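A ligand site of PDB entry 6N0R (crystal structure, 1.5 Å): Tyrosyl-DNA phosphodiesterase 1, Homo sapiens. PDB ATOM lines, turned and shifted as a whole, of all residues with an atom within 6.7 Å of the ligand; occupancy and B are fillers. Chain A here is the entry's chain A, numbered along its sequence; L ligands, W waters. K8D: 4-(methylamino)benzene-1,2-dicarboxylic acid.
The side-chain hydroxyl of Ser 252 lies within hydrogen-bond range of an oxygen (O12) of the ligand (2.8 Å). The side-chain amide nitrogen (ND2) of Asn 136 is in hydrogen-bond range of an oxygen (O09) of the ligand. NE2 of His 116 is in hydrogen-bond range of O13 of the ligand (2.8 Å). NZ of Lys 118 lies within salt-bridge range of O08 of the ligand, at 2.6 Å. O13 of the ligand is in salt-bridge range of NZ of Lys 348 (3.1 Å). NE2 of His 346 sits at hydrogen-bond distance from O09 of the ligand (2.5 Å). The side-chain amide nitrogen (ND2) of Asn 369 lies within hydrogen-bond range of an oxygen (O13) of the ligand, 3.2 Å away.
O of His 346 lies within hydrogen-bond range of NZ of Lys 348 (2.4 Å). The side-chain amide oxygen (OD1) of Asn 369 lies within hydrogen-bond range of the backbone NH (N) of Ser 252. OD1 of Asn 369 sits at hydrogen-bond distance from N of Ser 253 (3.1 Å). A ring nitrogen (ND1) of His 346 lies within hydrogen-bond range of the backbone carbonyl oxygen (O) of Thr 134, 2.8 Å away. The backbone carbonyl oxygen (O) of Pro 314 sits at hydrogen-bond distance from the side-chain hydroxyl (OG) of Ser 253, at 3.3 Å. ND1 of His 116 sits close to O of Ser 367 (2.9 Å). NZ of Lys 348 is in hydrogen-bond range of OG of Ser 252 (2.5 Å). OD1 of Asn 136 sits close to OD1 of Asn 56.
Tyr 57 touches the ligand (CB to O08, 3.5 Å). OG of Ser 253 touches C01 of the ligand, at 3.8 Å. O of Ser 312 touches O12 of the ligand (3.9 Å). Pro 314 touches the ligand. Within 4 Å of the ligand: Tyr 57, His 116, Lys 118, Asn 136, Ser 252, Ser 253, Ser 312, Pro 314, His 346, Lys 348 and Asn 369. The nearest printed residue that does not touch the ligand is Thr 114 (4.7 Å).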
ATOM      1  N   ASN A  56      19.931  36.370 -20.737  1.00  0.00           N
ATOM      2  CA  ASN A  56      20.888  35.326 -21.120  1.00  0.00           C
ATOM      3  C   ASN A  56      22.199  35.947 -21.594  1.00  0.00           C
ATOM      4  O   ASN A  56      22.400  37.163 -21.577  1.00  0.00           O
ATOM      5  CB  ASN A  56      20.300  34.386 -22.184  1.00  0.00           C
ATOM      6  CG  ASN A  56      20.684  32.925 -21.919  1.00  0.00           C
ATOM      7  OD1 ASN A  56      21.853  32.578 -22.026  1.00  0.00           O
ATOM      8  ND2 ASN A  56      19.723  32.093 -21.526  1.00  0.00           N
ATOM      9  N   TYR A  57      23.113  35.061 -21.998  1.00  0.00           N
ATOM     10  CA  TYR A  57      24.390  35.443 -22.560  1.00  0.00           C
ATOM     11  C   TYR A  57      24.390  35.388 -24.083  1.00  0.00           C
ATOM     12  O   TYR A  57      24.706  36.386 -24.745  1.00  0.00           O
ATOM     13  CB  TYR A  57      25.501  34.543 -21.988  1.00  0.00           C
ATOM     14  CG  TYR A  57      26.824  34.776 -22.672  1.00  0.00           C
ATOM     15  CD1 TYR A  57      27.526  35.949 -22.443  1.00  0.00           C
ATOM     16  CD2 TYR A  57      27.353  33.842 -23.555  1.00  0.00           C
ATOM     17  CE1 TYR A  57      28.737  36.180 -23.077  1.00  0.00           C
ATOM     18  CE2 TYR A  57      28.552  34.079 -24.194  1.00  0.00           C
ATOM     19  CZ  TYR A  57      29.234  35.244 -23.945  1.00  0.00           C
ATOM     20  OH  TYR A  57      30.442  35.478 -24.570  1.00  0.00           O
ATOM     21  N   CYS A  58      24.010  34.229 -24.641  1.00  0.00           N
ATOM     22  CA  CYS A  58      24.023  33.956 -26.075  1.00  0.00           C
ATOM     23  C   CYS A  58      22.614  33.636 -26.554  1.00  0.00           C
ATOM     24  O   CYS A  58      21.884  32.902 -25.878  1.00  0.00           O
ATOM     25  CB  CYS A  58      24.980  32.798 -26.406  1.00  0.00           C
ATOM     26  SG  CYS A  58      25.204  32.461 -28.168  1.00  0.00           S
ATOM     27  N   THR A 114      30.671  40.001 -17.758  1.00  0.00           N
ATOM     28  CA  THR A 114      29.781  39.252 -18.636  1.00  0.00           C
ATOM     29  C   THR A 114      28.366  39.296 -18.082  1.00  0.00           C
ATOM     30  O   THR A 114      28.181  39.191 -16.863  1.00  0.00           O
ATOM     31  CB  THR A 114      30.233  37.782 -18.732  1.00  0.00           C
ATOM     32  OG1 THR A 114      31.587  37.726 -19.188  1.00  0.00           O
ATOM     33  CG2 THR A 114      29.347  36.983 -19.679  1.00  0.00           C
ATOM     34  N   HIS A 115      27.359  39.426 -18.958  1.00  0.00           N
ATOM     35  CA  HIS A 115      25.978  39.230 -18.518  1.00  0.00           C
ATOM     36  C   HIS A 115      25.697  37.732 -18.641  1.00  0.00           C
ATOM     37  O   HIS A 115      25.306  37.230 -19.690  1.00  0.00           O
ATOM     38  CB  HIS A 115      24.980  40.043 -19.326  1.00  0.00           C
ATOM     39  CG  HIS A 115      23.582  39.897 -18.810  1.00  0.00           C
ATOM     40  ND1 HIS A 115      22.701  38.957 -19.294  1.00  0.00           N
ATOM     41  CD2 HIS A 115      22.956  40.506 -17.772  1.00  0.00           C
ATOM     42  CE1 HIS A 115      21.569  39.030 -18.605  1.00  0.00           C
ATOM     43  NE2 HIS A 115      21.696  39.963 -17.683  1.00  0.00           N
ATOM     44  N   HIS A 116      25.885  37.027 -17.535  1.00  0.00           N
ATOM     45  CA  HIS A 116      25.865  35.572 -17.555  1.00  0.00           C
ATOM     46  C   HIS A 116      24.551  34.975 -17.046  1.00  0.00           C
ATOM     47  O   HIS A 116      24.258  33.816 -17.344  1.00  0.00           O
ATOM     48  CB  HIS A 116      27.054  35.060 -16.730  1.00  0.00           C
ATOM     49  CG  HIS A 116      27.493  33.689 -17.091  1.00  0.00           C
ATOM     50  ND1 HIS A 116      27.527  32.667 -16.173  1.00  0.00           N
ATOM     51  CD2 HIS A 116      27.897  33.155 -18.274  1.00  0.00           C
ATOM     52  CE1 HIS A 116      27.935  31.557 -16.774  1.00  0.00           C
ATOM     53  NE2 HIS A 116      28.173  31.828 -18.039  1.00  0.00           N
ATOM     54  N   LYS A 118      20.953  33.552 -16.500  1.00  0.00           N
ATOM     55  CA  LYS A 118      19.979  32.880 -17.349  1.00  0.00           C
ATOM     56  C   LYS A 118      18.659  32.767 -16.598  1.00  0.00           C
ATOM     57  O   LYS A 118      18.540  32.036 -15.601  1.00  0.00           O
ATOM     58  CB  LYS A 118      20.501  31.512 -17.790  1.00  0.00           C
ATOM     59  CG  LYS A 118      21.659  31.670 -18.748  1.00  0.00           C
ATOM     60  CD  LYS A 118      22.763  30.732 -18.447  1.00  0.00           C
ATOM     61  CE  LYS A 118      23.803  30.787 -19.539  1.00  0.00           C
ATOM     62  NZ  LYS A 118      24.817  31.810 -19.248  1.00  0.00           N
ATOM     63  N   THR A 134      20.367  27.392 -16.464  1.00  0.00           N
ATOM     64  CA  THR A 134      21.779  27.473 -16.823  1.00  0.00           C
ATOM     65  C   THR A 134      22.067  27.438 -18.316  1.00  0.00           C
ATOM     66  O   THR A 134      23.253  27.500 -18.692  1.00  0.00           O
ATOM     67  CB  THR A 134      22.585  26.338 -16.135  1.00  0.00           C
ATOM     68  OG1 THR A 134      22.167  25.050 -16.625  1.00  0.00           O
ATOM     69  CG2 THR A 134      22.370  26.370 -14.623  1.00  0.00           C
ATOM     70  N   SER A 135      21.056  27.398 -19.188  1.00  0.00           N
ATOM     71  CA  SER A 135      21.286  27.203 -20.618  1.00  0.00           C
ATOM     72  C   SER A 135      21.231  28.511 -21.402  1.00  0.00           C
ATOM     73  O   SER A 135      20.366  29.349 -21.175  1.00  0.00           O
ATOM     74  CB  SER A 135      20.270  26.240 -21.246  1.00  0.00           C
ATOM     75  OG  SER A 135      20.156  25.032 -20.506  1.00  0.00           O
ATOM     76  N   ASN A 136      22.135  28.636 -22.366  1.00  0.00           N
ATOM     77  CA  ASN A 136      22.009  29.652 -23.392  1.00  0.00           C
ATOM     78  C   ASN A 136      20.805  29.344 -24.282  1.00  0.00           C
ATOM     79  O   ASN A 136      20.297  28.220 -24.318  1.00  0.00           O
ATOM     80  CB  ASN A 136      23.297  29.732 -24.226  1.00  0.00           C
ATOM     81  CG  ASN A 136      24.459  30.275 -23.417  1.00  0.00           C
ATOM     82  OD1 ASN A 136      24.598  31.493 -23.242  1.00  0.00           O
ATOM     83  ND2 ASN A 136      25.286  29.381 -22.894  1.00  0.00           N
ATOM     84  N   ASP A 141      22.609  24.057 -26.524  1.00  0.00           N
ATOM     85  CA  ASP A 141      22.597  24.041 -25.055  1.00  0.00           C
ATOM     86  C   ASP A 141      21.444  23.212 -24.491  1.00  0.00           C
ATOM     87  O   ASP A 141      21.484  22.849 -23.323  1.00  0.00           O
ATOM     88  CB  ASP A 141      22.532  25.464 -24.490  1.00  0.00           C
ATOM     89  CG  ASP A 141      23.913  26.000 -24.146  1.00  0.00           C
ATOM     90  OD1 ASP A 141      24.873  25.712 -24.900  1.00  0.00           O
ATOM     91  OD2 ASP A 141      24.042  26.670 -23.099  1.00  0.00           O
ATOM     92  N   PHE A 251      31.251  23.020 -12.195  1.00  0.00           N
ATOM     93  CA  PHE A 251      31.218  24.200 -13.059  1.00  0.00           C
ATOM     94  C   PHE A 251      31.712  23.849 -14.458  1.00  0.00           C
ATOM     95  O   PHE A 251      32.276  22.780 -14.699  1.00  0.00           O
ATOM     96  CB  PHE A 251      32.074  25.321 -12.449  1.00  0.00           C
ATOM     97  CG  PHE A 251      33.386  24.813 -11.943  1.00  0.00           C
ATOM     98  CD1 PHE A 251      34.451  24.635 -12.829  1.00  0.00           C
ATOM     99  CD2 PHE A 251      33.543  24.426 -10.619  1.00  0.00           C
ATOM    100  CE1 PHE A 251      35.648  24.116 -12.402  1.00  0.00           C
ATOM    101  CE2 PHE A 251      34.746  23.889 -10.184  1.00  0.00           C
ATOM    102  CZ  PHE A 251      35.800  23.742 -11.072  1.00  0.00           C
ATOM    103  N   SER A 252      31.491  24.772 -15.397  1.00  0.00           N
ATOM    104  CA  SER A 252      31.862  24.558 -16.786  1.00  0.00           C
ATOM    105  C   SER A 252      32.986  25.470 -17.266  1.00  0.00           C
ATOM    106  O   SER A 252      33.448  25.301 -18.398  1.00  0.00           O
ATOM    107  CB  SER A 252      30.641  24.704 -17.709  1.00  0.00           C
ATOM    108  OG  SER A 252      30.094  26.004 -17.653  1.00  0.00           O
ATOM    109  N   SER A 253      33.448  26.394 -16.443  1.00  0.00           N
ATOM    110  CA  SER A 253      34.535  27.289 -16.828  1.00  0.00           C
ATOM    111  C   SER A 253      35.297  27.665 -15.569  1.00  0.00           C
ATOM    112  O   SER A 253      34.752  27.653 -14.459  1.00  0.00           O
ATOM    113  CB  SER A 253      33.997  28.551 -17.539  1.00  0.00           C
ATOM    114  OG  SER A 253      35.073  29.332 -18.028  1.00  0.00           O
ATOM    115  N   VAL A 254      36.580  27.989 -15.740  1.00  0.00           N
ATOM    116  CA  VAL A 254      37.485  28.315 -14.646  1.00  0.00           C
ATOM    117  C   VAL A 254      38.191  29.613 -14.981  1.00  0.00           C
ATOM    118  O   VAL A 254      38.743  29.755 -16.080  1.00  0.00           O
ATOM    119  CB  VAL A 254      38.528  27.208 -14.409  1.00  0.00           C
ATOM    120  CG1 VAL A 254      39.258  27.445 -13.109  1.00  0.00           C
ATOM    121  CG2 VAL A 254      37.876  25.821 -14.432  1.00  0.00           C
ATOM    122  N   SER A 312      31.919  24.583 -25.221  1.00  0.00           N
ATOM    123  CA  SER A 312      31.139  25.156 -24.132  1.00  0.00           C
ATOM    124  C   SER A 312      31.809  24.938 -22.775  1.00  0.00           C
ATOM    125  O   SER A 312      31.160  25.060 -21.726  1.00  0.00           O
ATOM    126  CB  SER A 312      29.731  24.583 -24.144  1.00  0.00           C
ATOM    127  OG  SER A 312      29.068  24.889 -25.378  1.00  0.00           O
ATOM    128  N   LEU A 313      33.089  24.575 -22.784  1.00  0.00           N
ATOM    129  CA  LEU A 313      33.908  24.413 -21.584  1.00  0.00           C
ATOM    130  C   LEU A 313      35.132  25.303 -21.760  1.00  0.00           C
ATOM    131  O   LEU A 313      36.226  24.818 -22.087  1.00  0.00           O
ATOM    132  CB  LEU A 313      34.310  22.948 -21.368  1.00  0.00           C
ATOM    133  CG  LEU A 313      33.123  22.011 -21.090  1.00  0.00           C
ATOM    134  CD1 LEU A 313      33.486  20.552 -21.364  1.00  0.00           C
ATOM    135  CD2 LEU A 313      32.612  22.156 -19.657  1.00  0.00           C
ATOM    136  N   PRO A 314      34.973  26.615 -21.604  1.00  0.00           N
ATOM    137  CA  PRO A 314      36.051  27.555 -22.039  1.00  0.00           C
ATOM    138  C   PRO A 314      37.169  27.851 -21.035  1.00  0.00           C
ATOM    139  O   PRO A 314      37.265  28.923 -20.428  1.00  0.00           O
ATOM    140  CB  PRO A 314      35.255  28.833 -22.340  1.00  0.00           C
ATOM    141  CG  PRO A 314      34.119  28.777 -21.423  1.00  0.00           C
ATOM    142  CD  PRO A 314      33.750  27.325 -21.213  1.00  0.00           C
ATOM    143  N   HIS A 346      26.828  21.828 -18.403  1.00  0.00           N
ATOM    144  CA  HIS A 346      26.859  23.273 -18.442  1.00  0.00           C
ATOM    145  C   HIS A 346      26.117  23.850 -17.237  1.00  0.00           C
ATOM    146  O   HIS A 346      26.172  25.070 -16.997  1.00  0.00           O
ATOM    147  CB  HIS A 346      26.263  23.759 -19.777  1.00  0.00           C
ATOM    148  CG  HIS A 346      26.395  25.228 -20.018  1.00  0.00           C
ATOM    149  ND1 HIS A 346      25.374  26.114 -19.780  1.00  0.00           N
ATOM    150  CD2 HIS A 346      27.425  25.960 -20.511  1.00  0.00           C
ATOM    151  CE1 HIS A 346      25.770  27.341 -20.090  1.00  0.00           C
ATOM    152  NE2 HIS A 346      27.009  27.276 -20.538  1.00  0.00           N
ATOM    153  N   LYS A 348      25.890  24.595 -13.272  1.00  0.00           N
ATOM    154  CA  LYS A 348      26.860  24.871 -12.209  1.00  0.00           C
ATOM    155  C   LYS A 348      26.141  24.646 -10.893  1.00  0.00           C
ATOM    156  O   LYS A 348      25.015  25.117 -10.711  1.00  0.00           O
ATOM    157  CB  LYS A 348      27.396  26.308 -12.254  1.00  0.00           C
ATOM    158  CG  LYS A 348      28.088  26.731 -13.559  1.00  0.00           C
ATOM    159  CD  LYS A 348      27.087  27.233 -14.595  1.00  0.00           C
ATOM    160  CE  LYS A 348      27.805  27.771 -15.836  1.00  0.00           C
ATOM    161  NZ  LYS A 348      27.869  26.778 -16.930  1.00  0.00           N
ATOM    162  N   SER A 367      24.245  30.225 -12.361  1.00  0.00           N
ATOM    163  CA  SER A 367      25.054  30.453 -13.547  1.00  0.00           C
ATOM    164  C   SER A 367      26.531  30.629 -13.218  1.00  0.00           C
ATOM    165  O   SER A 367      27.334  30.609 -14.157  1.00  0.00           O
ATOM    166  CB  SER A 367      24.614  31.697 -14.315  1.00  0.00           C
ATOM    167  OG  SER A 367      24.570  32.835 -13.451  1.00  0.00           O
ATOM    168  N   ASN A 369      30.279  30.271 -12.565  1.00  0.00           N
ATOM    169  CA  ASN A 369      31.414  29.356 -12.688  1.00  0.00           C
ATOM    170  C   ASN A 369      32.445  29.661 -11.600  1.00  0.00           C
ATOM    171  O   ASN A 369      32.261  30.536 -10.754  1.00  0.00           O
ATOM    172  CB  ASN A 369      32.033  29.498 -14.076  1.00  0.00           C
ATOM    173  CG  ASN A 369      31.244  28.795 -15.131  1.00  0.00           C
ATOM    174  OD1 ASN A 369      30.939  27.611 -14.999  1.00  0.00           O
ATOM    175  ND2 ASN A 369      30.891  29.500 -16.200  1.00  0.00           N
ATOM    176  N   SER A 371      35.036  31.429 -10.718  1.00  0.00           N
ATOM    177  CA  SER A 371      35.790  32.611 -11.120  1.00  0.00           C
ATOM    178  C   SER A 371      35.539  33.797 -10.182  1.00  0.00           C
ATOM    179  O   SER A 371      34.446  33.953  -9.621  1.00  0.00           O
ATOM    180  CB  SER A 371      35.462  33.008 -12.565  1.00  0.00           C
ATOM    181  OG  SER A 371      34.329  33.831 -12.638  1.00  0.00           O
ATOM    182  N   TRP A 443      40.326  24.203 -23.877  1.00  0.00           N
ATOM    183  CA  TRP A 443      39.594  24.229 -25.139  1.00  0.00           C
ATOM    184  C   TRP A 443      40.428  24.723 -26.325  1.00  0.00           C
ATOM    185  O   TRP A 443      40.014  24.501 -27.467  1.00  0.00           O
ATOM    186  CB  TRP A 443      38.330  25.090 -25.028  1.00  0.00           C
ATOM    187  CG  TRP A 443      38.509  26.593 -24.953  1.00  0.00           C
ATOM    188  CD1 TRP A 443      39.632  27.283 -24.596  1.00  0.00           C
ATOM    189  CD2 TRP A 443      37.513  27.588 -25.248  1.00  0.00           C
ATOM    190  NE1 TRP A 443      39.396  28.642 -24.648  1.00  0.00           N
ATOM    191  CE2 TRP A 443      38.101  28.852 -25.046  1.00  0.00           C
ATOM    192  CE3 TRP A 443      36.177  27.528 -25.670  1.00  0.00           C
ATOM    193  CZ2 TRP A 443      37.409  30.045 -25.248  1.00  0.00           C
ATOM    194  CZ3 TRP A 443      35.488  28.712 -25.869  1.00  0.00           C
ATOM    195  CH2 TRP A 443      36.105  29.952 -25.663  1.00  0.00           C
HETATM  196  C10 K8D L   1      30.288  30.509 -19.978  1.00  0.00           C
HETATM  197  C01 K8D L   1      33.932  32.817 -18.964  1.00  0.00           C
HETATM  198  C03 K8D L   1      32.013  32.104 -20.441  1.00  0.00           C
HETATM  199  C04 K8D L   1      31.122  32.864 -21.182  1.00  0.00           C
HETATM  200  C05 K8D L   1      29.801  32.447 -21.313  1.00  0.00           C
HETATM  201  C06 K8D L   1      29.380  31.254 -20.718  1.00  0.00           C
HETATM  202  C07 K8D L   1      27.918  30.820 -20.867  1.00  0.00           C
HETATM  203  C11 K8D L   1      29.852  29.204 -19.293  1.00  0.00           C
HETATM  204  C14 K8D L   1      31.594  30.936 -19.842  1.00  0.00           C
HETATM  205  N02 K8D L   1      33.402  32.530 -20.285  1.00  0.00           N
HETATM  206  O08 K8D L   1      27.011  31.677 -20.701  1.00  0.00           O
HETATM  207  O09 K8D L   1      27.612  29.645 -21.195  1.00  0.00           O
HETATM  208  O12 K8D L   1      30.541  28.154 -19.390  1.00  0.00           O
HETATM  209  O13 K8D L   1      28.808  29.210 -18.614  1.00  0.00           O
HETATM  210  O   HOH W   1      31.849  32.127 -16.578  1.00  0.00           O
